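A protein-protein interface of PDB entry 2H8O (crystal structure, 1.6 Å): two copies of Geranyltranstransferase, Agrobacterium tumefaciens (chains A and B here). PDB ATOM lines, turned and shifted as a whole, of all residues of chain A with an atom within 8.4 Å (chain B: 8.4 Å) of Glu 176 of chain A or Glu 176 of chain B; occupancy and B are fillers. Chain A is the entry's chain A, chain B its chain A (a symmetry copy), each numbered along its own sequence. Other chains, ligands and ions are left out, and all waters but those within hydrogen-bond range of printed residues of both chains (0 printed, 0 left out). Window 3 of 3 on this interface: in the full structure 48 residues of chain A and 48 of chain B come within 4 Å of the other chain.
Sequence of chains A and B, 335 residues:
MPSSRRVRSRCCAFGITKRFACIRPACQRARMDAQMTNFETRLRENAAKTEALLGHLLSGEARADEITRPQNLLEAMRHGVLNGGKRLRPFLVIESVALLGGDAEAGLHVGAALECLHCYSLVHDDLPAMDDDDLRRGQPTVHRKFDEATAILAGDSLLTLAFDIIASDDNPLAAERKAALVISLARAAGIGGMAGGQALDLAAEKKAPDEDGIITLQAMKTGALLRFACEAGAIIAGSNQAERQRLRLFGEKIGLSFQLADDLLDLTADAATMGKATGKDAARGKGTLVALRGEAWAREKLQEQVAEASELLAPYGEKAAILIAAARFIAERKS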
ATOM      1  N   ALA A 167      -5.730 -19.685  -9.524  1.00  0.00           N
ATOM      2  CA  ALA A 167      -6.643 -19.395  -8.414  1.00  0.00           C
ATOM      3  C   ALA A 167      -6.744 -17.911  -8.077  1.00  0.00           C
ATOM      4  O   ALA A 167      -7.665 -17.504  -7.360  1.00  0.00           O
ATOM      5  CB  ALA A 167      -6.228 -20.204  -7.164  1.00  0.00           C
ATOM      6  N   ASP A 169      -7.143 -13.848  -7.807  1.00  0.00           N
ATOM      7  CA  ASP A 169      -8.277 -12.979  -8.049  1.00  0.00           C
ATOM      8  C   ASP A 169      -8.175 -12.249  -9.381  1.00  0.00           C
ATOM      9  O   ASP A 169      -9.210 -11.861  -9.933  1.00  0.00           O
ATOM     10  CB  ASP A 169      -8.432 -11.959  -6.928  1.00  0.00           C
ATOM     11  CG  ASP A 169      -8.868 -12.573  -5.615  1.00  0.00           C
ATOM     12  OD1 ASP A 169      -9.358 -13.726  -5.564  1.00  0.00           O
ATOM     13  OD2 ASP A 169      -8.703 -11.865  -4.597  1.00  0.00           O
ATOM     14  N   LEU A 173     -12.650 -15.497 -12.955  1.00  0.00           N
ATOM     15  CA  LEU A 173     -13.306 -16.796 -13.028  1.00  0.00           C
ATOM     16  C   LEU A 173     -13.858 -17.179 -11.642  1.00  0.00           C
ATOM     17  O   LEU A 173     -13.207 -16.955 -10.628  1.00  0.00           O
ATOM     18  CB  LEU A 173     -12.297 -17.828 -13.509  1.00  0.00           C
ATOM     19  CG  LEU A 173     -12.799 -19.216 -13.866  1.00  0.00           C
ATOM     20  CD1 LEU A 173     -13.782 -19.127 -15.042  1.00  0.00           C
ATOM     21  CD2 LEU A 173     -11.604 -20.111 -14.196  1.00  0.00           C
ATOM     22  N   ALA A 174     -15.073 -17.722 -11.606  1.00  0.00           N
ATOM     23  CA  ALA A 174     -15.716 -18.081 -10.339  1.00  0.00           C
ATOM     24  C   ALA A 174     -14.882 -19.120  -9.593  1.00  0.00           C
ATOM     25  O   ALA A 174     -14.220 -19.954 -10.210  1.00  0.00           O
ATOM     26  CB  ALA A 174     -17.117 -18.616 -10.569  1.00  0.00           C
ATOM     27  N   ALA A 175     -14.951 -19.056  -8.269  1.00  0.00           N
ATOM     28  CA  ALA A 175     -14.187 -19.939  -7.378  1.00  0.00           C
ATOM     29  C   ALA A 175     -14.427 -21.416  -7.665  1.00  0.00           C
ATOM     30  O   ALA A 175     -13.508 -22.205  -7.646  1.00  0.00           O
ATOM     31  CB  ALA A 175     -14.500 -19.624  -5.908  1.00  0.00           C
ATOM     32  N   GLU A 176     -15.672 -21.783  -7.946  1.00  0.00           N
ATOM     33  CA  GLU A 176     -16.002 -23.184  -8.202  1.00  0.00           C
ATOM     34  C   GLU A 176     -15.270 -23.705  -9.438  1.00  0.00           C
ATOM     35  O   GLU A 176     -14.768 -24.838  -9.460  1.00  0.00           O
ATOM     36  CB  GLU A 176     -17.512 -23.358  -8.374  1.00  0.00           C
ATOM     37  CG  GLU A 176     -18.319 -23.064  -7.117  1.00  0.00           C
ATOM     38  CD  GLU A 176     -18.575 -21.559  -6.822  1.00  0.00           C
ATOM     39  OE1 GLU A 176     -18.243 -20.647  -7.639  1.00  0.00           O
ATOM     40  OE2 GLU A 176     -19.129 -21.297  -5.724  1.00  0.00           O
ATOM     41  N   ARG A 177     -15.175 -22.844 -10.455  1.00  0.00           N
ATOM     42  CA  ARG A 177     -14.462 -23.185 -11.683  1.00  0.00           C
ATOM     43  C   ARG A 177     -12.931 -23.229 -11.469  1.00  0.00           C
ATOM     44  O   ARG A 177     -12.240 -24.105 -12.007  1.00  0.00           O
ATOM     45  CB  ARG A 177     -14.863 -22.219 -12.801  1.00  0.00           C
ATOM     46  CG  ARG A 177     -16.310 -22.361 -13.201  1.00  0.00           C
ATOM     47  CD  ARG A 177     -16.721 -21.346 -14.252  1.00  0.00           C
ATOM     48  NE  ARG A 177     -18.173 -21.291 -14.376  1.00  0.00           N
ATOM     49  CZ  ARG A 177     -18.824 -20.586 -15.300  1.00  0.00           C
ATOM     50  NH1 ARG A 177     -18.165 -19.910 -16.231  1.00  0.00           N
ATOM     51  NH2 ARG A 177     -20.156 -20.590 -15.313  1.00  0.00           N
ATOM     52  N   LYS A 178     -12.415 -22.294 -10.675  1.00  0.00           N
ATOM     53  CA  LYS A 178     -11.005 -22.308 -10.249  1.00  0.00           C
ATOM     54  C   LYS A 178     -10.656 -23.610  -9.521  1.00  0.00           C
ATOM     55  O   LYS A 178      -9.678 -24.259  -9.850  1.00  0.00           O
ATOM     56  CB  LYS A 178     -10.710 -21.101  -9.364  1.00  0.00           C
ATOM     57  CG  LYS A 178     -10.628 -19.796 -10.169  1.00  0.00           C
ATOM     58  CD  LYS A 178     -10.610 -18.548  -9.292  1.00  0.00           C
ATOM     59  CE  LYS A 178     -10.062 -17.338 -10.070  1.00  0.00           C
ATOM     60  NZ  LYS A 178     -10.452 -16.038  -9.494  1.00  0.00           N
ATOM     61  N   ALA A 179     -11.478 -24.001  -8.555  1.00  0.00           N
ATOM     62  CA  ALA A 179     -11.234 -25.271  -7.825  1.00  0.00           C
ATOM     63  C   ALA A 179     -11.222 -26.458  -8.774  1.00  0.00           C
ATOM     64  O   ALA A 179     -10.344 -27.308  -8.704  1.00  0.00           O
ATOM     65  CB  ALA A 179     -12.254 -25.478  -6.701  1.00  0.00           C
ATOM     66  N   ALA A 180     -12.197 -26.507  -9.689  1.00  0.00           N
ATOM     67  CA  ALA A 180     -12.263 -27.591 -10.670  1.00  0.00           C
ATOM     68  C   ALA A 180     -11.008 -27.654 -11.529  1.00  0.00           C
ATOM     69  O   ALA A 180     -10.498 -28.725 -11.840  1.00  0.00           O
ATOM     70  CB  ALA A 180     -13.489 -27.413 -11.558  1.00  0.00           C
ATOM     71  N   LEU A 181     -10.505 -26.490 -11.924  1.00  0.00           N
ATOM     72  CA  LEU A 181      -9.292 -26.414 -12.728  1.00  0.00           C
ATOM     73  C   LEU A 181      -8.066 -26.849 -11.928  1.00  0.00           C
ATOM     74  O   LEU A 181      -7.173 -27.483 -12.479  1.00  0.00           O
ATOM     75  CB  LEU A 181      -9.075 -24.984 -13.211  1.00  0.00           C
ATOM     76  CG  LEU A 181      -9.975 -24.496 -14.343  1.00  0.00           C
ATOM     77  CD1 LEU A 181      -9.779 -23.014 -14.559  1.00  0.00           C
ATOM     78  CD2 LEU A 181      -9.701 -25.240 -15.618  1.00  0.00           C
ATOM     79  N   VAL A 182      -7.988 -26.465 -10.656  1.00  0.00           N
ATOM     80  CA  VAL A 182      -6.857 -26.855  -9.814  1.00  0.00           C
ATOM     81  C   VAL A 182      -6.813 -28.392  -9.708  1.00  0.00           C
ATOM     82  O   VAL A 182      -5.752 -29.017  -9.882  1.00  0.00           O
ATOM     83  CB  VAL A 182      -6.911 -26.201  -8.428  1.00  0.00           C
ATOM     84  CG1 VAL A 182      -5.851 -26.834  -7.473  1.00  0.00           C
ATOM     85  CG2 VAL A 182      -6.696 -24.654  -8.520  1.00  0.00           C
ATOM     86  N   ILE A 183      -7.966 -28.993  -9.458  1.00  0.00           N
ATOM     87  CA  ILE A 183      -8.062 -30.467  -9.397  1.00  0.00           C
ATOM     88  C   ILE A 183      -7.642 -31.065 -10.735  1.00  0.00           C
ATOM     89  O   ILE A 183      -6.799 -31.951 -10.795  1.00  0.00           O
ATOM     90  CB  ILE A 183      -9.488 -30.956  -9.005  1.00  0.00           C
ATOM     91  CG1 ILE A 183      -9.913 -30.428  -7.628  1.00  0.00           C
ATOM     92  CG2 ILE A 183      -9.579 -32.492  -9.066  1.00  0.00           C
ATOM     93  CD1 ILE A 183     -11.430 -30.492  -7.435  1.00  0.00           C
ATOM     94  N   ILE A 235     -14.534 -26.219 -18.677  1.00  0.00           N
ATOM     95  CA  ILE A 235     -14.611 -25.845 -17.263  1.00  0.00           C
ATOM     96  C   ILE A 235     -14.733 -24.316 -17.101  1.00  0.00           C
ATOM     97  O   ILE A 235     -15.575 -23.804 -16.348  1.00  0.00           O
ATOM     98  CB  ILE A 235     -13.388 -26.361 -16.478  1.00  0.00           C
ATOM     99  CG1 ILE A 235     -13.376 -27.883 -16.496  1.00  0.00           C
ATOM    100  CG2 ILE A 235     -13.424 -25.837 -15.050  1.00  0.00           C
ATOM    101  CD1 ILE A 235     -12.149 -28.451 -15.850  1.00  0.00           C
ATOM    102  N   ARG A 244     -18.262 -30.792 -21.536  1.00  0.00           N
ATOM    103  CA  ARG A 244     -16.959 -30.999 -20.904  1.00  0.00           C
ATOM    104  C   ARG A 244     -16.350 -32.339 -21.348  1.00  0.00           C
ATOM    105  O   ARG A 244     -15.188 -32.395 -21.720  1.00  0.00           O
ATOM    106  CB  ARG A 244     -17.081 -30.911 -19.390  1.00  0.00           C
ATOM    107  CG  ARG A 244     -15.782 -31.143 -18.671  1.00  0.00           C
ATOM    108  CD  ARG A 244     -15.880 -30.797 -17.220  1.00  0.00           C
ATOM    109  NE  ARG A 244     -14.701 -31.284 -16.500  1.00  0.00           N
ATOM    110  CZ  ARG A 244     -14.507 -31.133 -15.196  1.00  0.00           C
ATOM    111  NH1 ARG A 244     -15.385 -30.474 -14.442  1.00  0.00           N
ATOM    112  NH2 ARG A 244     -13.413 -31.650 -14.641  1.00  0.00           N
ATOM    113  N   ALA B 167      -7.881 -28.644  -3.094  1.00  0.00           N
ATOM    114  CA  ALA B 167      -9.015 -28.251  -3.937  1.00  0.00           C
ATOM    115  C   ALA B 167     -10.049 -29.357  -4.126  1.00  0.00           C
ATOM    116  O   ALA B 167     -11.167 -29.083  -4.576  1.00  0.00           O
ATOM    117  CB  ALA B 167      -8.505 -27.751  -5.308  1.00  0.00           C
ATOM    118  N   ASP B 169     -12.824 -32.360  -3.981  1.00  0.00           N
ATOM    119  CA  ASP B 169     -14.158 -32.404  -3.417  1.00  0.00           C
ATOM    120  C   ASP B 169     -14.202 -33.154  -2.092  1.00  0.00           C
ATOM    121  O   ASP B 169     -15.104 -32.895  -1.287  1.00  0.00           O
ATOM    122  CB  ASP B 169     -15.140 -33.045  -4.389  1.00  0.00           C
ATOM    123  CG  ASP B 169     -15.418 -32.193  -5.609  1.00  0.00           C
ATOM    124  OD1 ASP B 169     -15.125 -30.974  -5.634  1.00  0.00           O
ATOM    125  OD2 ASP B 169     -15.945 -32.780  -6.580  1.00  0.00           O
ATOM    126  N   LEU B 173     -14.909 -28.176   2.159  1.00  0.00           N
ATOM    127  CA  LEU B 173     -14.630 -26.751   2.281  1.00  0.00           C
ATOM    128  C   LEU B 173     -15.151 -26.010   1.035  1.00  0.00           C
ATOM    129  O   LEU B 173     -15.015 -26.496  -0.082  1.00  0.00           O
ATOM    130  CB  LEU B 173     -13.129 -26.557   2.434  1.00  0.00           C
ATOM    131  CG  LEU B 173     -12.612 -25.174   2.790  1.00  0.00           C
ATOM    132  CD1 LEU B 173     -13.152 -24.754   4.164  1.00  0.00           C
ATOM    133  CD2 LEU B 173     -11.084 -25.188   2.763  1.00  0.00           C
ATOM    134  N   ALA B 174     -15.775 -24.852   1.240  1.00  0.00           N
ATOM    135  CA  ALA B 174     -16.353 -24.086   0.132  1.00  0.00           C
ATOM    136  C   ALA B 174     -15.267 -23.688  -0.865  1.00  0.00           C
ATOM    137  O   ALA B 174     -14.119 -23.458  -0.484  1.00  0.00           O
ATOM    138  CB  ALA B 174     -17.065 -22.845   0.638  1.00  0.00           C
ATOM    139  N   ALA B 175     -15.665 -23.597  -2.128  1.00  0.00           N
ATOM    140  CA  ALA B 175     -14.758 -23.271  -3.237  1.00  0.00           C
ATOM    141  C   ALA B 175     -14.004 -21.965  -3.018  1.00  0.00           C
ATOM    142  O   ALA B 175     -12.831 -21.874  -3.309  1.00  0.00           O
ATOM    143  CB  ALA B 175     -15.527 -23.225  -4.565  1.00  0.00           C
ATOM    144  N   GLU B 176     -14.683 -20.956  -2.485  1.00  0.00           N
ATOM    145  CA  GLU B 176     -14.050 -19.656  -2.269  1.00  0.00           C
ATOM    146  C   GLU B 176     -12.890 -19.767  -1.279  1.00  0.00           C
ATOM    147  O   GLU B 176     -11.826 -19.157  -1.462  1.00  0.00           O
ATOM    148  CB  GLU B 176     -15.073 -18.637  -1.766  1.00  0.00           C
ATOM    149  CG  GLU B 176     -16.161 -18.298  -2.775  1.00  0.00           C
ATOM    150  CD  GLU B 176     -17.317 -19.332  -2.886  1.00  0.00           C
ATOM    151  OE1 GLU B 176     -17.412 -20.323  -2.100  1.00  0.00           O
ATOM    152  OE2 GLU B 176     -18.154 -19.129  -3.802  1.00  0.00           O
ATOM    153  N   ARG B 177     -13.090 -20.593  -0.249  1.00  0.00           N
ATOM    154  CA  ARG B 177     -12.053 -20.836   0.751  1.00  0.00           C
ATOM    155  C   ARG B 177     -10.895 -21.690   0.186  1.00  0.00           C
ATOM    156  O   ARG B 177      -9.719 -21.438   0.479  1.00  0.00           O
ATOM    157  CB  ARG B 177     -12.676 -21.460   2.002  1.00  0.00           C
ATOM    158  CG  ARG B 177     -13.617 -20.522   2.714  1.00  0.00           C
ATOM    159  CD  ARG B 177     -14.291 -21.174   3.907  1.00  0.00           C
ATOM    160  NE  ARG B 177     -15.417 -20.369   4.367  1.00  0.00           N
ATOM    161  CZ  ARG B 177     -16.123 -20.620   5.469  1.00  0.00           C
ATOM    162  NH1 ARG B 177     -15.798 -21.624   6.271  1.00  0.00           N
ATOM    163  NH2 ARG B 177     -17.146 -19.829   5.789  1.00  0.00           N
ATOM    164  N   LYS B 178     -11.233 -22.684  -0.632  1.00  0.00           N
ATOM    165  CA  LYS B 178     -10.235 -23.475  -1.373  1.00  0.00           C
ATOM    166  C   LYS B 178      -9.364 -22.580  -2.260  1.00  0.00           C
ATOM    167  O   LYS B 178      -8.148 -22.663  -2.218  1.00  0.00           O
ATOM    168  CB  LYS B 178     -10.926 -24.549  -2.206  1.00  0.00           C
ATOM    169  CG  LYS B 178     -11.449 -25.707  -1.343  1.00  0.00           C
ATOM    170  CD  LYS B 178     -12.376 -26.651  -2.102  1.00  0.00           C
ATOM    171  CE  LYS B 178     -12.489 -28.007  -1.380  1.00  0.00           C
ATOM    172  NZ  LYS B 178     -13.692 -28.774  -1.748  1.00  0.00           N
ATOM    173  N   ALA B 179      -9.991 -21.705  -3.036  1.00  0.00           N
ATOM    174  CA  ALA B 179      -9.220 -20.773  -3.900  1.00  0.00           C
ATOM    175  C   ALA B 179      -8.289 -19.902  -3.074  1.00  0.00           C
ATOM    176  O   ALA B 179      -7.124 -19.733  -3.411  1.00  0.00           O
ATOM    177  CB  ALA B 179     -10.145 -19.917  -4.769  1.00  0.00           C
ATOM    178  N   ALA B 180      -8.800 -19.356  -1.964  1.00  0.00           N
ATOM    179  CA  ALA B 180      -7.983 -18.523  -1.081  1.00  0.00           C
ATOM    180  C   ALA B 180      -6.778 -19.281  -0.544  1.00  0.00           C
ATOM    181  O   ALA B 180      -5.679 -18.748  -0.443  1.00  0.00           O
ATOM    182  CB  ALA B 180      -8.829 -18.010   0.077  1.00  0.00           C
ATOM    183  N   LEU B 181      -6.986 -20.544  -0.188  1.00  0.00           N
ATOM    184  CA  LEU B 181      -5.908 -21.385   0.317  1.00  0.00           C
ATOM    185  C   LEU B 181      -4.890 -21.699  -0.776  1.00  0.00           C
ATOM    186  O   LEU B 181      -3.697 -21.761  -0.498  1.00  0.00           O
ATOM    187  CB  LEU B 181      -6.475 -22.698   0.846  1.00  0.00           C
ATOM    188  CG  LEU B 181      -7.197 -22.644   2.190  1.00  0.00           C
ATOM    189  CD1 LEU B 181      -7.872 -23.966   2.468  1.00  0.00           C
ATOM    190  CD2 LEU B 181      -6.250 -22.309   3.305  1.00  0.00           C
ATOM    191  N   VAL B 182      -5.351 -21.955  -1.998  1.00  0.00           N
ATOM    192  CA  VAL B 182      -4.442 -22.247  -3.107  1.00  0.00           C
ATOM    193  C   VAL B 182      -3.524 -21.031  -3.338  1.00  0.00           C
ATOM    194  O   VAL B 182      -2.294 -21.171  -3.463  1.00  0.00           O
ATOM    195  CB  VAL B 182      -5.192 -22.632  -4.387  1.00  0.00           C
ATOM    196  CG1 VAL B 182      -4.220 -22.678  -5.608  1.00  0.00           C
ATOM    197  CG2 VAL B 182      -5.919 -24.008  -4.228  1.00  0.00           C
ATOM    198  N   ILE B 183      -4.116 -19.846  -3.360  1.00  0.00           N
ATOM    199  CA  ILE B 183      -3.333 -18.603  -3.511  1.00  0.00           C
ATOM    200  C   ILE B 183      -2.344 -18.475  -2.357  1.00  0.00           C
ATOM    201  O   ILE B 183      -1.155 -18.267  -2.562  1.00  0.00           O
ATOM    202  CB  ILE B 183      -4.234 -17.337  -3.598  1.00  0.00           C
ATOM    203  CG1 ILE B 183      -5.194 -17.402  -4.795  1.00  0.00           C
ATOM    204  CG2 ILE B 183      -3.382 -16.054  -3.637  1.00  0.00           C
ATOM    205  CD1 ILE B 183      -6.372 -16.439  -4.635  1.00  0.00           C
ATOM    206  N   ILE B 235      -8.695 -18.899   7.315  1.00  0.00           N
ATOM    207  CA  ILE B 235      -9.303 -19.044   5.990  1.00  0.00           C
ATOM    208  C   ILE B 235     -10.339 -20.186   5.980  1.00  0.00           C
ATOM    209  O   ILE B 235     -11.467 -20.041   5.484  1.00  0.00           O
ATOM    210  CB  ILE B 235      -8.235 -19.293   4.907  1.00  0.00           C
ATOM    211  CG1 ILE B 235      -7.321 -18.081   4.804  1.00  0.00           C
ATOM    212  CG2 ILE B 235      -8.903 -19.582   3.571  1.00  0.00           C
ATOM    213  CD1 ILE B 235      -6.187 -18.301   3.850  1.00  0.00           C
ATOM    214  N   ARG B 244      -8.206 -13.245  10.597  1.00  0.00           N
ATOM    215  CA  ARG B 244      -7.223 -13.801   9.667  1.00  0.00           C
ATOM    216  C   ARG B 244      -5.857 -13.120   9.853  1.00  0.00           C
ATOM    217  O   ARG B 244      -4.841 -13.791   9.940  1.00  0.00           O
ATOM    218  CB  ARG B 244      -7.720 -13.682   8.234  1.00  0.00           C
ATOM    219  CG  ARG B 244      -6.747 -14.209   7.218  1.00  0.00           C
ATOM    220  CD  ARG B 244      -7.363 -14.317   5.860  1.00  0.00           C
ATOM    221  NE  ARG B 244      -6.331 -14.568   4.852  1.00  0.00           N
ATOM    222  CZ  ARG B 244      -6.572 -14.703   3.554  1.00  0.00           C
ATOM    223  NH1 ARG B 244      -7.815 -14.654   3.076  1.00  0.00           N
ATOM    224  NH2 ARG B 244      -5.550 -14.892   2.722  1.00  0.00           N
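Ala 167 of chain A touches Ala 179 of chain B. Val 182 of chain B touches Ala 167 of chain A. Ile 183 of chain B touches Ala 167 of chain A (CD1 to O, 3.2 Å). Ala 175 of chain A touches Ala 175 of chain B. Glu 176 of chain B touches Ala 175 of chain A. Glu 176 of chain A touches Ala 175 of chain B (CA to CB, 3.7 Å). Ala 179 of chain A touches Ala 167 of chain B. Val 182 of chain A touches Ala 167 of chain B. CD1 of Ile 183 of chain A touches O of Ala 167 of chain B (3.2 Å).
Of the printed residues of chain B, Ala 167 of chain A touches Ala 179, Val 182 and Ile 183. Of chain B, only Ala 175 (3.8 Å) and Glu 176 (3.7 Å) come within 4 Å of Ala 175 of chain A. Glu 176 of chain A touches just these residues of chain B: Ala 175 (3.7 Å) and Glu 176 (3.1 Å). Printed residues of chain B within 4 Å of Ala 179 of chain A: Ala 167. Of chain A, only Ala 175 and Glu 176 come within 4 Å of Glu 176 of chain B. Of the printed residues of chain A, Ala 179 of chain B touches Ala 167 (3.9 Å). Ala 180 of chain B touches none of the printed residues of chain A. Of the printed residues of chain A, Val 182 of chain B touches Ala 167. The nearest printed residue of chain B that does not touch Glu 176 of chain A is Ala 179 of chain B (6.6 Å). The nearest printed residue of chain A that does not touch Glu 176 of chain B is Ala 179 of chain A (6.6 Å). The nearest printed residue of chain A that does not touch Ala 167 of chain B is Ala 180 of chain A (5.8 Å).
Ala 167 of chain A touches Val 182 of chain B, and with the chains exchanged Val 182 of chain A touches Ala 167 of chain B. Ala 167 of chain A touches Ile 183 of chain B, and with the chains exchanged Ile 183 of chain A touches Ala 167 of chain B. Ala 175 of chain B touches its own counterpart, Ala 175 of chain A. Glu 176 of chain A touches its own counterpart, Glu 176 of chain B. Of the 10 pairs that touch across the chains among the printed residues, 10 have their exchanged pair printed and touching as well.
Of the 15 printed residues of chain A, 6 touch a printed residue of chain B. Hydrophobic or aromatic side chains of chain A that line the printed part of chain B: Ala 167, Ala 175, Val 182 and Ile 183. Printed residues of chain B that touch a printed residue of chain A: Ala 167, Ala 175, Glu 176, Ala 179, Val 182 and Ile 183. Hydrophobic or aromatic side chains of chain B that line the printed part of chain A: Ala 167, Ala 175, Val 182 and Ile 183. Among the printed residues, 10 pairs touch across the chains. Among the printed residues, no Asp or Glu carboxylate lies within 4 Å of a Lys or Arg side-chain nitrogen of the other chain.
The side-chain carboxylate (OE2) of Glu 176 of chain A lies close to the side-chain carboxylate (OE2) of Glu 176 of chain B, 3.1 Å away.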
